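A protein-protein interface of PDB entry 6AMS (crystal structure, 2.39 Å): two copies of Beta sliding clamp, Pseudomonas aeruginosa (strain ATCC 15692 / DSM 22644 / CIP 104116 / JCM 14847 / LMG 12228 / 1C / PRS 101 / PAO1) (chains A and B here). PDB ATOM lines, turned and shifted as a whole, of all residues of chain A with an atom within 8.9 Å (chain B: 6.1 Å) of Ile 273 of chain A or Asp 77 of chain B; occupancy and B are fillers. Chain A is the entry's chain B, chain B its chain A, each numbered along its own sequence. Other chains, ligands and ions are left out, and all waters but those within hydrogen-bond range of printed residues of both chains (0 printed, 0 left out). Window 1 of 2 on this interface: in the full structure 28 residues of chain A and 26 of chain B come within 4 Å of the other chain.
The backbone carbonyl oxygen (O) of Ala 303 of chain A lies within hydrogen-bond range of the backbone NH (N) of Ala 295 of chain A (2.9 Å).
The backbone NH of Asn 297 of chain A lies within hydrogen-bond range of the backbone carbonyl oxygen of Leu 274 of chain A (3.3 Å).
The side-chain amide nitrogen (ND2) of Asn 297 of chain A lies within hydrogen-bond range of the side-chain carboxylate (OE1) of Glu 301 of chain A, 2.8 Å away.
The side-chain amide oxygen (OD1) of Asn 297 of chain A sits at hydrogen-bond distance from the backbone NH (N) of Glu 299 of chain A, 3.1 Å away.
OE2 of Glu 302 of chain A sits close to OD1 of Asn 296 of chain A (3.1 Å).
O of Ile 78 of chain B sits at hydrogen-bond distance from OG of Ser 81 of chain B (2.9 Å).
Of the printed residues of chain B, Arg 270 of chain A touches Ser 81, Leu 82 and Phe 106.
Of chain B, only Asp 77 (3.6 Å) and Ser 81 (3.8 Å) come within 4 Å of Ile 273 of chain A.
Printed residues of chain B within 4 Å of Leu 274 of chain A: Phe 106 (3.9 Å).
Asn 296 of chain A touches none of the printed residues of chain B.
Glu 305 of chain A touches none of the printed residues of chain B.
Of chain A, only Ile 273 comes within 4 Å of Asp 77 of chain B.
The nearest residue of chain B that does not touch Ile 273 of chain A is Ile 78 of chain B (4.1 Å).
The nearest residue of chain A that does not touch Asp 77 of chain B is Arg 270 of chain A (6.2 Å).
The nearest printed residue of chain A that does not touch Ser 81 of chain B is Glu 266 of chain A (5.2 Å).
Among the printed residues, merely in contact across the chains: Arg 270 of chain A with Leu 82 of chain B (3.8 Å), Arg 270 of chain A with Phe 106 of chain B (3.6 Å), Ile 273 of chain A with Asp 77 of chain B (3.6 Å), Ile 273 of chain A with Ser 81 of chain B (3.8 Å), Leu 274 of chain A with Phe 106 of chain B (3.9 Å), Asn 297 of chain A with Lys 74 of chain B (3.9 Å), Glu 302 of chain A with Phe 106 of chain B (3.3 Å) and Ala 303 of chain A with Phe 106 of chain B (3.7 Å).
Printed residues of chain A that touch a printed residue of chain B: Arg 270, Ile 273, Leu 274, Asn 297, Glu 299, Glu 301, Glu 302 and Ala 303.
Hydrophobic or aromatic side chains of chain A within 4 Å of the printed part of chain B: Ile 273, Leu 274 and Ala 303.
Of the 13 printed residues of chain B, 5 touch a printed residue of chain A.
Hydrophobic or aromatic side chains of chain B within 4 Å of the printed part of chain A: Leu 82 and Phe 106.
The side-chain amino group of Lys 74 of chain B is in salt-bridge range of the side-chain carboxylate of Glu 301 of chain A (2.8 Å).
The side-chain amino group (NZ) of Lys 74 of chain B lies within salt-bridge range of the side-chain carboxylate (OE1) of Glu 299 of chain A, at 3.3 Å.
NH1 of Arg 270 of chain A is in hydrogen-bond range of O of Ser 81 of chain B (2.8 Å).
No position is printed for both chains.
Of the 11 pairs that touch across the chains among the printed residues, none has its exchanged pair printed and touching as well.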
ATOM      1  N   GLU A 266     -14.333   1.018 -19.607  1.00  0.00           N
ATOM      2  CA  GLU A 266     -14.483   2.413 -19.241  1.00  0.00           C
ATOM      3  C   GLU A 266     -15.654   3.072 -19.958  1.00  0.00           C
ATOM      4  O   GLU A 266     -16.396   3.811 -19.326  1.00  0.00           O
ATOM      5  CB  GLU A 266     -13.167   3.189 -19.487  1.00  0.00           C
ATOM      6  CG  GLU A 266     -12.069   2.865 -18.473  1.00  0.00           C
ATOM      7  CD  GLU A 266     -10.661   3.294 -18.933  1.00  0.00           C
ATOM      8  OE1 GLU A 266     -10.497   3.709 -20.096  1.00  0.00           O
ATOM      9  OE2 GLU A 266      -9.685   3.180 -18.146  1.00  0.00           O
ATOM     10  N   ALA A 267     -15.847   2.782 -21.247  1.00  0.00           N
ATOM     11  CA  ALA A 267     -16.977   3.327 -22.011  1.00  0.00           C
ATOM     12  C   ALA A 267     -18.340   2.749 -21.594  1.00  0.00           C
ATOM     13  O   ALA A 267     -19.364   3.443 -21.608  1.00  0.00           O
ATOM     14  CB  ALA A 267     -16.773   3.081 -23.493  1.00  0.00           C
ATOM     15  N   PHE A 268     -18.363   1.466 -21.266  1.00  0.00           N
ATOM     16  CA  PHE A 268     -19.579   0.873 -20.740  1.00  0.00           C
ATOM     17  C   PHE A 268     -19.892   1.417 -19.343  1.00  0.00           C
ATOM     18  O   PHE A 268     -21.055   1.665 -19.088  1.00  0.00           O
ATOM     19  CB  PHE A 268     -19.527  -0.665 -20.729  1.00  0.00           C
ATOM     20  CG  PHE A 268     -19.621  -1.301 -22.090  1.00  0.00           C
ATOM     21  CD1 PHE A 268     -20.548  -0.881 -23.024  1.00  0.00           C
ATOM     22  CD2 PHE A 268     -18.793  -2.366 -22.419  1.00  0.00           C
ATOM     23  CE1 PHE A 268     -20.651  -1.489 -24.253  1.00  0.00           C
ATOM     24  CE2 PHE A 268     -18.876  -2.983 -23.669  1.00  0.00           C
ATOM     25  CZ  PHE A 268     -19.814  -2.547 -24.587  1.00  0.00           C
ATOM     26  N   SER A 269     -18.905   1.610 -18.453  1.00  0.00           N
ATOM     27  CA  SER A 269     -19.263   2.138 -17.104  1.00  0.00           C
ATOM     28  C   SER A 269     -19.660   3.612 -17.151  1.00  0.00           C
ATOM     29  O   SER A 269     -20.552   4.022 -16.414  1.00  0.00           O
ATOM     30  CB  SER A 269     -18.243   1.861 -15.981  1.00  0.00           C
ATOM     31  OG  SER A 269     -16.899   1.890 -16.409  1.00  0.00           O
ATOM     32  N   ARG A 270     -19.074   4.362 -18.050  1.00  0.00           N
ATOM     33  CA  ARG A 270     -19.427   5.742 -18.210  1.00  0.00           C
ATOM     34  C   ARG A 270     -20.853   5.862 -18.683  1.00  0.00           C
ATOM     35  O   ARG A 270     -21.591   6.607 -18.126  1.00  0.00           O
ATOM     36  CB  ARG A 270     -18.549   6.407 -19.231  1.00  0.00           C
ATOM     37  CG  ARG A 270     -17.335   7.067 -18.689  1.00  0.00           C
ATOM     38  CD  ARG A 270     -16.638   7.922 -19.713  1.00  0.00           C
ATOM     39  NE  ARG A 270     -15.956   7.165 -20.725  1.00  0.00           N
ATOM     40  CZ  ARG A 270     -14.714   6.769 -20.626  1.00  0.00           C
ATOM     41  NH1 ARG A 270     -14.021   7.045 -19.568  1.00  0.00           N
ATOM     42  NH2 ARG A 270     -14.177   6.097 -21.587  1.00  0.00           N
ATOM     43  N   THR A 271     -21.225   5.112 -19.717  1.00  0.00           N
ATOM     44  CA  THR A 271     -22.572   5.175 -20.247  1.00  0.00           C
ATOM     45  C   THR A 271     -23.573   4.546 -19.276  1.00  0.00           C
ATOM     46  O   THR A 271     -24.719   4.963 -19.237  1.00  0.00           O
ATOM     47  CB  THR A 271     -22.698   4.540 -21.636  1.00  0.00           C
ATOM     48  OG1 THR A 271     -22.354   3.158 -21.573  1.00  0.00           O
ATOM     49  CG2 THR A 271     -21.805   5.240 -22.621  1.00  0.00           C
ATOM     50  N   ALA A 272     -23.130   3.561 -18.485  1.00  0.00           N
ATOM     51  CA  ALA A 272     -23.995   2.878 -17.496  1.00  0.00           C
ATOM     52  C   ALA A 272     -24.642   3.843 -16.524  1.00  0.00           C
ATOM     53  O   ALA A 272     -25.776   3.642 -16.128  1.00  0.00           O
ATOM     54  CB  ALA A 272     -23.220   1.825 -16.715  1.00  0.00           C
ATOM     55  N   ILE A 273     -23.914   4.900 -16.188  1.00  0.00           N
ATOM     56  CA  ILE A 273     -24.376   5.918 -15.245  1.00  0.00           C
ATOM     57  C   ILE A 273     -25.763   6.478 -15.609  1.00  0.00           C
ATOM     58  O   ILE A 273     -26.548   6.782 -14.722  1.00  0.00           O
ATOM     59  CB  ILE A 273     -23.341   7.056 -15.107  1.00  0.00           C
ATOM     60  CG1 ILE A 273     -22.055   6.531 -14.433  1.00  0.00           C
ATOM     61  CG2 ILE A 273     -23.895   8.210 -14.270  1.00  0.00           C
ATOM     62  CD1 ILE A 273     -20.834   7.357 -14.780  1.00  0.00           C
ATOM     63  N   LEU A 274     -26.055   6.609 -16.902  1.00  0.00           N
ATOM     64  CA  LEU A 274     -27.317   7.152 -17.331  1.00  0.00           C
ATOM     65  C   LEU A 274     -28.242   6.102 -17.944  1.00  0.00           C
ATOM     66  O   LEU A 274     -29.212   6.435 -18.615  1.00  0.00           O
ATOM     67  CB  LEU A 274     -27.059   8.290 -18.299  1.00  0.00           C
ATOM     68  CG  LEU A 274     -26.345   9.518 -17.716  1.00  0.00           C
ATOM     69  CD1 LEU A 274     -26.256  10.615 -18.760  1.00  0.00           C
ATOM     70  CD2 LEU A 274     -27.065  10.056 -16.485  1.00  0.00           C
ATOM     71  N   SER A 275     -27.977   4.826 -17.660  1.00  0.00           N
ATOM     72  CA  SER A 275     -28.863   3.759 -18.077  1.00  0.00           C
ATOM     73  C   SER A 275     -29.912   3.604 -17.007  1.00  0.00           C
ATOM     74  O   SER A 275     -29.722   4.064 -15.887  1.00  0.00           O
ATOM     75  CB  SER A 275     -28.113   2.446 -18.277  1.00  0.00           C
ATOM     76  OG  SER A 275     -27.606   1.926 -17.065  1.00  0.00           O
ATOM     77  N   ASN A 276     -31.029   2.969 -17.368  1.00  0.00           N
ATOM     78  CA  ASN A 276     -32.094   2.648 -16.428  1.00  0.00           C
ATOM     79  C   ASN A 276     -31.505   1.889 -15.218  1.00  0.00           C
ATOM     80  O   ASN A 276     -30.820   0.882 -15.383  1.00  0.00           O
ATOM     81  CB  ASN A 276     -33.170   1.852 -17.162  1.00  0.00           C
ATOM     82  CG  ASN A 276     -34.461   1.700 -16.365  1.00  0.00           C
ATOM     83  OD1 ASN A 276     -34.490   1.050 -15.332  1.00  0.00           O
ATOM     84  ND2 ASN A 276     -35.549   2.234 -16.887  1.00  0.00           N
ATOM     85  N   GLU A 277     -31.750   2.379 -14.008  1.00  0.00           N
ATOM     86  CA  GLU A 277     -31.121   1.810 -12.817  1.00  0.00           C
ATOM     87  C   GLU A 277     -31.539   0.374 -12.526  1.00  0.00           C
ATOM     88  O   GLU A 277     -30.749  -0.374 -11.944  1.00  0.00           O
ATOM     89  CB  GLU A 277     -31.348   2.720 -11.621  1.00  0.00           C
ATOM     90  CG  GLU A 277     -30.616   4.059 -11.796  1.00  0.00           C
ATOM     91  CD  GLU A 277     -31.123   5.190 -10.911  1.00  0.00           C
ATOM     92  OE1 GLU A 277     -31.956   4.894 -10.012  1.00  0.00           O
ATOM     93  OE2 GLU A 277     -30.663   6.349 -11.143  1.00  0.00           O
ATOM     94  N   ARG A 280     -31.006  -1.457 -16.930  1.00  0.00           N
ATOM     95  CA  ARG A 280     -29.593  -1.306 -17.251  1.00  0.00           C
ATOM     96  C   ARG A 280     -29.321  -1.476 -18.743  1.00  0.00           C
ATOM     97  O   ARG A 280     -28.300  -2.029 -19.142  1.00  0.00           O
ATOM     98  CB  ARG A 280     -28.738  -2.267 -16.379  1.00  0.00           C
ATOM     99  CG  ARG A 280     -28.758  -1.972 -14.880  1.00  0.00           C
ATOM    100  CD  ARG A 280     -27.872  -0.752 -14.527  1.00  0.00           C
ATOM    101  NE  ARG A 280     -26.448  -1.093 -14.561  1.00  0.00           N
ATOM    102  CZ  ARG A 280     -25.461  -0.262 -14.243  1.00  0.00           C
ATOM    103  NH1 ARG A 280     -25.722   0.985 -13.882  1.00  0.00           N
ATOM    104  NH2 ARG A 280     -24.194  -0.684 -14.281  1.00  0.00           N
ATOM    105  N   GLY A 281     -30.229  -0.958 -19.553  1.00  0.00           N
ATOM    106  CA  GLY A 281     -30.185  -1.110 -21.001  1.00  0.00           C
ATOM    107  C   GLY A 281     -29.204  -0.141 -21.667  1.00  0.00           C
ATOM    108  O   GLY A 281     -29.251   1.034 -21.414  1.00  0.00           O
ATOM    109  N   ILE A 282     -28.339  -0.680 -22.515  1.00  0.00           N
ATOM    110  CA  ILE A 282     -27.496   0.085 -23.399  1.00  0.00           C
ATOM    111  C   ILE A 282     -27.787  -0.356 -24.843  1.00  0.00           C
ATOM    112  O   ILE A 282     -28.167  -1.495 -25.097  1.00  0.00           O
ATOM    113  CB  ILE A 282     -25.992   0.148 -22.995  1.00  0.00           C
ATOM    114  CG1 ILE A 282     -25.310  -1.199 -22.791  1.00  0.00           C
ATOM    115  CG2 ILE A 282     -25.792   0.991 -21.750  1.00  0.00           C
ATOM    116  CD1 ILE A 282     -24.928  -1.846 -24.094  1.00  0.00           C
ATOM    117  N   ALA A 295     -26.967   5.203 -23.897  1.00  0.00           N
ATOM    118  CA  ALA A 295     -27.734   4.850 -22.701  1.00  0.00           C
ATOM    119  C   ALA A 295     -28.754   5.931 -22.471  1.00  0.00           C
ATOM    120  O   ALA A 295     -28.383   7.107 -22.478  1.00  0.00           O
ATOM    121  CB  ALA A 295     -26.840   4.725 -21.489  1.00  0.00           C
ATOM    122  N   ASN A 296     -30.010   5.530 -22.258  1.00  0.00           N
ATOM    123  CA  ASN A 296     -31.097   6.455 -21.890  1.00  0.00           C
ATOM    124  C   ASN A 296     -31.784   5.980 -20.628  1.00  0.00           C
ATOM    125  O   ASN A 296     -31.882   4.764 -20.405  1.00  0.00           O
ATOM    126  CB  ASN A 296     -32.125   6.524 -22.998  1.00  0.00           C
ATOM    127  CG  ASN A 296     -31.549   7.091 -24.258  1.00  0.00           C
ATOM    128  OD1 ASN A 296     -31.534   8.315 -24.462  1.00  0.00           O
ATOM    129  ND2 ASN A 296     -31.111   6.208 -25.135  1.00  0.00           N
ATOM    130  N   ASN A 297     -32.263   6.918 -19.802  1.00  0.00           N
ATOM    131  CA  ASN A 297     -33.047   6.552 -18.611  1.00  0.00           C
ATOM    132  C   ASN A 297     -34.461   7.173 -18.666  1.00  0.00           C
ATOM    133  O   ASN A 297     -34.761   7.894 -19.622  1.00  0.00           O
ATOM    134  CB  ASN A 297     -32.260   6.842 -17.321  1.00  0.00           C
ATOM    135  CG  ASN A 297     -32.009   8.324 -17.067  1.00  0.00           C
ATOM    136  OD1 ASN A 297     -32.712   9.199 -17.588  1.00  0.00           O
ATOM    137  ND2 ASN A 297     -31.025   8.601 -16.214  1.00  0.00           N
ATOM    138  N   GLU A 299     -35.691   9.638 -16.925  1.00  0.00           N
ATOM    139  CA  GLU A 299     -35.586  11.106 -16.862  1.00  0.00           C
ATOM    140  C   GLU A 299     -35.066  11.799 -18.179  1.00  0.00           C
ATOM    141  O   GLU A 299     -34.665  12.984 -18.161  1.00  0.00           O
ATOM    142  CB  GLU A 299     -34.712  11.514 -15.665  1.00  0.00           C
ATOM    143  CG  GLU A 299     -35.328  11.198 -14.299  1.00  0.00           C
ATOM    144  CD  GLU A 299     -34.414  11.545 -13.142  1.00  0.00           C
ATOM    145  OE1 GLU A 299     -33.210  11.862 -13.344  1.00  0.00           O
ATOM    146  OE2 GLU A 299     -34.890  11.420 -11.977  1.00  0.00           O
ATOM    147  N   GLU A 301     -32.323  11.417 -19.769  1.00  0.00           N
ATOM    148  CA  GLU A 301     -30.909  11.685 -19.750  1.00  0.00           C
ATOM    149  C   GLU A 301     -30.271  10.707 -20.735  1.00  0.00           C
ATOM    150  O   GLU A 301     -30.820   9.627 -20.983  1.00  0.00           O
ATOM    151  CB  GLU A 301     -30.366  11.558 -18.315  1.00  0.00           C
ATOM    152  CG  GLU A 301     -30.965  12.604 -17.369  1.00  0.00           C
ATOM    153  CD  GLU A 301     -30.594  12.428 -15.903  1.00  0.00           C
ATOM    154  OE1 GLU A 301     -30.496  11.269 -15.435  1.00  0.00           O
ATOM    155  OE2 GLU A 301     -30.447  13.454 -15.189  1.00  0.00           O
ATOM    156  N   GLU A 302     -29.145  11.100 -21.323  1.00  0.00           N
ATOM    157  CA  GLU A 302     -28.500  10.303 -22.352  1.00  0.00           C
ATOM    158  C   GLU A 302     -27.000  10.336 -22.209  1.00  0.00           C
ATOM    159  O   GLU A 302     -26.432  11.387 -22.065  1.00  0.00           O
ATOM    160  CB  GLU A 302     -28.859  10.823 -23.738  1.00  0.00           C
ATOM    161  CG  GLU A 302     -28.608   9.801 -24.824  1.00  0.00           C
ATOM    162  CD  GLU A 302     -29.042  10.288 -26.205  1.00  0.00           C
ATOM    163  OE1 GLU A 302     -28.201  10.910 -26.865  1.00  0.00           O
ATOM    164  OE2 GLU A 302     -30.179  10.040 -26.659  1.00  0.00           O
ATOM    165  N   ALA A 303     -26.358   9.181 -22.289  1.00  0.00           N
ATOM    166  CA  ALA A 303     -24.913   9.117 -22.446  1.00  0.00           C
ATOM    167  C   ALA A 303     -24.638   8.472 -23.792  1.00  0.00           C
ATOM    168  O   ALA A 303     -25.301   7.510 -24.149  1.00  0.00           O
ATOM    169  CB  ALA A 303     -24.300   8.305 -21.323  1.00  0.00           C
ATOM    170  N   GLU A 305     -21.304   7.353 -26.438  1.00  0.00           N
ATOM    171  CA  GLU A 305     -19.877   7.146 -26.507  1.00  0.00           C
ATOM    172  C   GLU A 305     -19.472   6.316 -27.715  1.00  0.00           C
ATOM    173  O   GLU A 305     -20.149   5.407 -28.090  1.00  0.00           O
ATOM    174  CB  GLU A 305     -19.351   6.550 -25.200  1.00  0.00           C
ATOM    175  CG  GLU A 305     -17.891   6.226 -25.175  1.00  0.00           C
ATOM    176  CD  GLU A 305     -17.270   6.575 -23.890  1.00  0.00           C
ATOM    177  OE1 GLU A 305     -17.987   6.951 -22.978  1.00  0.00           O
ATOM    178  OE2 GLU A 305     -16.062   6.472 -23.809  1.00  0.00           O
ATOM    179  N   VAL A 322     -26.001  -3.756 -19.470  1.00  0.00           N
ATOM    180  CA  VAL A 322     -24.608  -3.286 -19.434  1.00  0.00           C
ATOM    181  C   VAL A 322     -23.854  -3.870 -18.240  1.00  0.00           C
ATOM    182  O   VAL A 322     -22.630  -3.971 -18.282  1.00  0.00           O
ATOM    183  CB  VAL A 322     -24.495  -1.735 -19.460  1.00  0.00           C
ATOM    184  CG1 VAL A 322     -24.939  -1.095 -18.135  1.00  0.00           C
ATOM    185  CG2 VAL A 322     -23.063  -1.280 -19.801  1.00  0.00           C
ATOM    186  N   LEU A 326     -20.214  -5.656 -18.388  1.00  0.00           N
ATOM    187  CA  LEU A 326     -19.155  -5.316 -17.409  1.00  0.00           C
ATOM    188  C   LEU A 326     -18.698  -6.481 -16.553  1.00  0.00           C
ATOM    189  O   LEU A 326     -17.527  -6.532 -16.209  1.00  0.00           O
ATOM    190  CB  LEU A 326     -19.606  -4.195 -16.478  1.00  0.00           C
ATOM    191  CG  LEU A 326     -19.727  -2.843 -17.160  1.00  0.00           C
ATOM    192  CD1 LEU A 326     -20.459  -1.879 -16.248  1.00  0.00           C
ATOM    193  CD2 LEU A 326     -18.348  -2.300 -17.518  1.00  0.00           C
ATOM    194  N   LEU B  14     -16.410  19.480  -6.651  1.00  0.00           N
ATOM    195  CA  LEU B  14     -17.610  18.681  -6.851  1.00  0.00           C
ATOM    196  C   LEU B  14     -17.663  17.512  -5.882  1.00  0.00           C
ATOM    197  O   LEU B  14     -18.725  17.209  -5.362  1.00  0.00           O
ATOM    198  CB  LEU B  14     -17.676  18.232  -8.299  1.00  0.00           C
ATOM    199  CG  LEU B  14     -18.910  17.545  -8.808  1.00  0.00           C
ATOM    200  CD1 LEU B  14     -20.144  18.408  -8.546  1.00  0.00           C
ATOM    201  CD2 LEU B  14     -18.729  17.285 -10.305  1.00  0.00           C
ATOM    202  N   ALA B  72     -26.165  15.884  -8.336  1.00  0.00           N
ATOM    203  CA  ALA B  72     -24.792  16.020  -7.842  1.00  0.00           C
ATOM    204  C   ALA B  72     -24.020  14.743  -8.004  1.00  0.00           C
ATOM    205  O   ALA B  72     -22.960  14.744  -8.632  1.00  0.00           O
ATOM    206  CB  ALA B  72     -24.802  16.440  -6.383  1.00  0.00           C
ATOM    207  N   ARG B  73     -24.546  13.669  -7.428  1.00  0.00           N
ATOM    208  CA  ARG B  73     -23.969  12.324  -7.547  1.00  0.00           C
ATOM    209  C   ARG B  73     -23.707  12.014  -9.053  1.00  0.00           C
ATOM    210  O   ARG B  73     -22.596  11.659  -9.412  1.00  0.00           O
ATOM    211  CB  ARG B  73     -24.942  11.271  -6.973  1.00  0.00           C
ATOM    212  CG  ARG B  73     -25.063  11.198  -5.505  1.00  0.00           C
ATOM    213  CD  ARG B  73     -23.885  10.418  -4.942  1.00  0.00           C
ATOM    214  NE  ARG B  73     -23.438  11.083  -3.729  1.00  0.00           N
ATOM    215  CZ  ARG B  73     -22.331  10.776  -3.024  1.00  0.00           C
ATOM    216  NH1 ARG B  73     -21.501   9.792  -3.423  1.00  0.00           N
ATOM    217  NH2 ARG B  73     -22.064  11.485  -1.922  1.00  0.00           N
ATOM    218  N   LYS B  74     -24.699  12.202  -9.932  1.00  0.00           N
ATOM    219  CA  LYS B  74     -24.516  11.858 -11.338  1.00  0.00           C
ATOM    220  C   LYS B  74     -23.441  12.701 -12.021  1.00  0.00           C
ATOM    221  O   LYS B  74     -22.658  12.154 -12.789  1.00  0.00           O
ATOM    222  CB  LYS B  74     -25.823  11.939 -12.129  1.00  0.00           C
ATOM    223  CG  LYS B  74     -26.686  10.695 -12.038  1.00  0.00           C
ATOM    224  CD  LYS B  74     -28.055  10.960 -12.632  1.00  0.00           C
ATOM    225  CE  LYS B  74     -29.061   9.888 -12.265  1.00  0.00           C
ATOM    226  NZ  LYS B  74     -30.405  10.301 -12.778  1.00  0.00           N
ATOM    227  N   LEU B  75     -23.383  14.010 -11.754  1.00  0.00           N
ATOM    228  CA  LEU B  75     -22.336  14.850 -12.349  1.00  0.00           C
ATOM    229  C   LEU B  75     -20.976  14.393 -11.857  1.00  0.00           C
ATOM    230  O   LEU B  75     -20.035  14.322 -12.643  1.00  0.00           O
ATOM    231  CB  LEU B  75     -22.512  16.367 -12.033  1.00  0.00           C
ATOM    232  CG  LEU B  75     -21.510  17.316 -12.731  1.00  0.00           C
ATOM    233  CD1 LEU B  75     -21.489  17.132 -14.238  1.00  0.00           C
ATOM    234  CD2 LEU B  75     -21.812  18.758 -12.400  1.00  0.00           C
ATOM    235  N   MET B  76     -20.874  14.103 -10.555  1.00  0.00           N
ATOM    236  CA  MET B  76     -19.602  13.709  -9.962  1.00  0.00           C
ATOM    237  C   MET B  76     -19.155  12.380 -10.530  1.00  0.00           C
ATOM    238  O   MET B  76     -18.022  12.254 -10.917  1.00  0.00           O
ATOM    239  CB  MET B  76     -19.705  13.609  -8.440  1.00  0.00           C
ATOM    240  CG  MET B  76     -18.413  13.144  -7.751  1.00  0.00           C
ATOM    241  SD  MET B  76     -18.549  13.033  -5.941  1.00  0.00           S
ATOM    242  CE  MET B  76     -19.706  11.619  -5.805  1.00  0.00           C
ATOM    243  N   ASP B  77     -20.044  11.393 -10.573  1.00  0.00           N
ATOM    244  CA  ASP B  77     -19.738  10.082 -11.169  1.00  0.00           C
ATOM    245  C   ASP B  77     -19.310  10.199 -12.635  1.00  0.00           C
ATOM    246  O   ASP B  77     -18.422   9.474 -13.070  1.00  0.00           O
ATOM    247  CB  ASP B  77     -20.929   9.124 -11.101  1.00  0.00           C
ATOM    248  CG  ASP B  77     -21.261   8.686  -9.675  1.00  0.00           C
ATOM    249  OD1 ASP B  77     -20.459   8.898  -8.740  1.00  0.00           O
ATOM    250  OD2 ASP B  77     -22.369   8.156  -9.477  1.00  0.00           O
ATOM    251  N   ILE B  78     -19.957  11.077 -13.392  1.00  0.00           N
ATOM    252  CA  ILE B  78     -19.585  11.284 -14.771  1.00  0.00           C
ATOM    253  C   ILE B  78     -18.178  11.885 -14.812  1.00  0.00           C
ATOM    254  O   ILE B  78     -17.336  11.412 -15.529  1.00  0.00           O
ATOM    255  CB  ILE B  78     -20.600  12.177 -15.511  1.00  0.00           C
ATOM    256  CG1 ILE B  78     -21.921  11.468 -15.687  1.00  0.00           C
ATOM    257  CG2 ILE B  78     -20.091  12.549 -16.894  1.00  0.00           C
ATOM    258  CD1 ILE B  78     -23.057  12.441 -15.948  1.00  0.00           C
ATOM    259  N   CYS B  79     -17.928  12.895 -13.998  1.00  0.00           N
ATOM    260  CA  CYS B  79     -16.632  13.556 -13.952  1.00  0.00           C
ATOM    261  C   CYS B  79     -15.501  12.601 -13.484  1.00  0.00           C
ATOM    262  O   CYS B  79     -14.396  12.619 -14.017  1.00  0.00           O
ATOM    263  CB  CYS B  79     -16.729  14.783 -13.045  1.00  0.00           C
ATOM    264  SG  CYS B  79     -15.290  15.870 -13.078  1.00  0.00           S
ATOM    265  N   LYS B  80     -15.809  11.773 -12.498  1.00  0.00           N
ATOM    266  CA  LYS B  80     -14.872  10.786 -11.944  1.00  0.00           C
ATOM    267  C   LYS B  80     -14.459   9.791 -13.025  1.00  0.00           C
ATOM    268  O   LYS B  80     -13.280   9.530 -13.209  1.00  0.00           O
ATOM    269  CB  LYS B  80     -15.537  10.045 -10.748  1.00  0.00           C
ATOM    270  CG  LYS B  80     -14.679   9.097  -9.925  1.00  0.00           C
ATOM    271  CD  LYS B  80     -13.404   9.749  -9.385  1.00  0.00           C
ATOM    272  CE  LYS B  80     -12.640   8.756  -8.505  1.00  0.00           C
ATOM    273  NZ  LYS B  80     -11.835   7.746  -9.273  1.00  0.00           N
ATOM    274  N   SER B  81     -15.442   9.292 -13.765  1.00  0.00           N
ATOM    275  CA  SER B  81     -15.230   8.220 -14.738  1.00  0.00           C
ATOM    276  C   SER B  81     -14.556   8.647 -16.026  1.00  0.00           C
ATOM    277  O   SER B  81     -14.237   7.794 -16.839  1.00  0.00           O
ATOM    278  CB  SER B  81     -16.571   7.608 -15.110  1.00  0.00           C
ATOM    279  OG  SER B  81     -17.351   8.550 -15.836  1.00  0.00           O
ATOM    280  N   LEU B  82     -14.387   9.930 -16.238  1.00  0.00           N
ATOM    281  CA  LEU B  82     -13.730  10.418 -17.415  1.00  0.00           C
ATOM    282  C   LEU B  82     -12.236  10.214 -17.338  1.00  0.00           C
ATOM    283  O   LEU B  82     -11.670  10.035 -16.291  1.00  0.00           O
ATOM    284  CB  LEU B  82     -14.074  11.876 -17.657  1.00  0.00           C
ATOM    285  CG  LEU B  82     -15.508  12.196 -18.069  1.00  0.00           C
ATOM    286  CD1 LEU B  82     -15.787  13.662 -17.992  1.00  0.00           C
ATOM    287  CD2 LEU B  82     -15.804  11.648 -19.441  1.00  0.00           C
ATOM    288  N   PHE B 106     -22.903  13.574 -22.570  1.00  0.00           N
ATOM    289  CA  PHE B 106     -23.860  13.334 -21.509  1.00  0.00           C
ATOM    290  C   PHE B 106     -24.912  14.426 -21.457  1.00  0.00           C
ATOM    291  O   PHE B 106     -24.617  15.600 -21.636  1.00  0.00           O
ATOM    292  CB  PHE B 106     -23.158  13.264 -20.154  1.00  0.00           C
ATOM    293  CG  PHE B 106     -22.109  12.201 -20.064  1.00  0.00           C
ATOM    294  CD1 PHE B 106     -20.818  12.451 -20.481  1.00  0.00           C
ATOM    295  CD2 PHE B 106     -22.414  10.958 -19.559  1.00  0.00           C
ATOM    296  CE1 PHE B 106     -19.852  11.477 -20.401  1.00  0.00           C
ATOM    297  CE2 PHE B 106     -21.453   9.978 -19.472  1.00  0.00           C
ATOM    298  CZ  PHE B 106     -20.169  10.236 -19.894  1.00  0.00           C
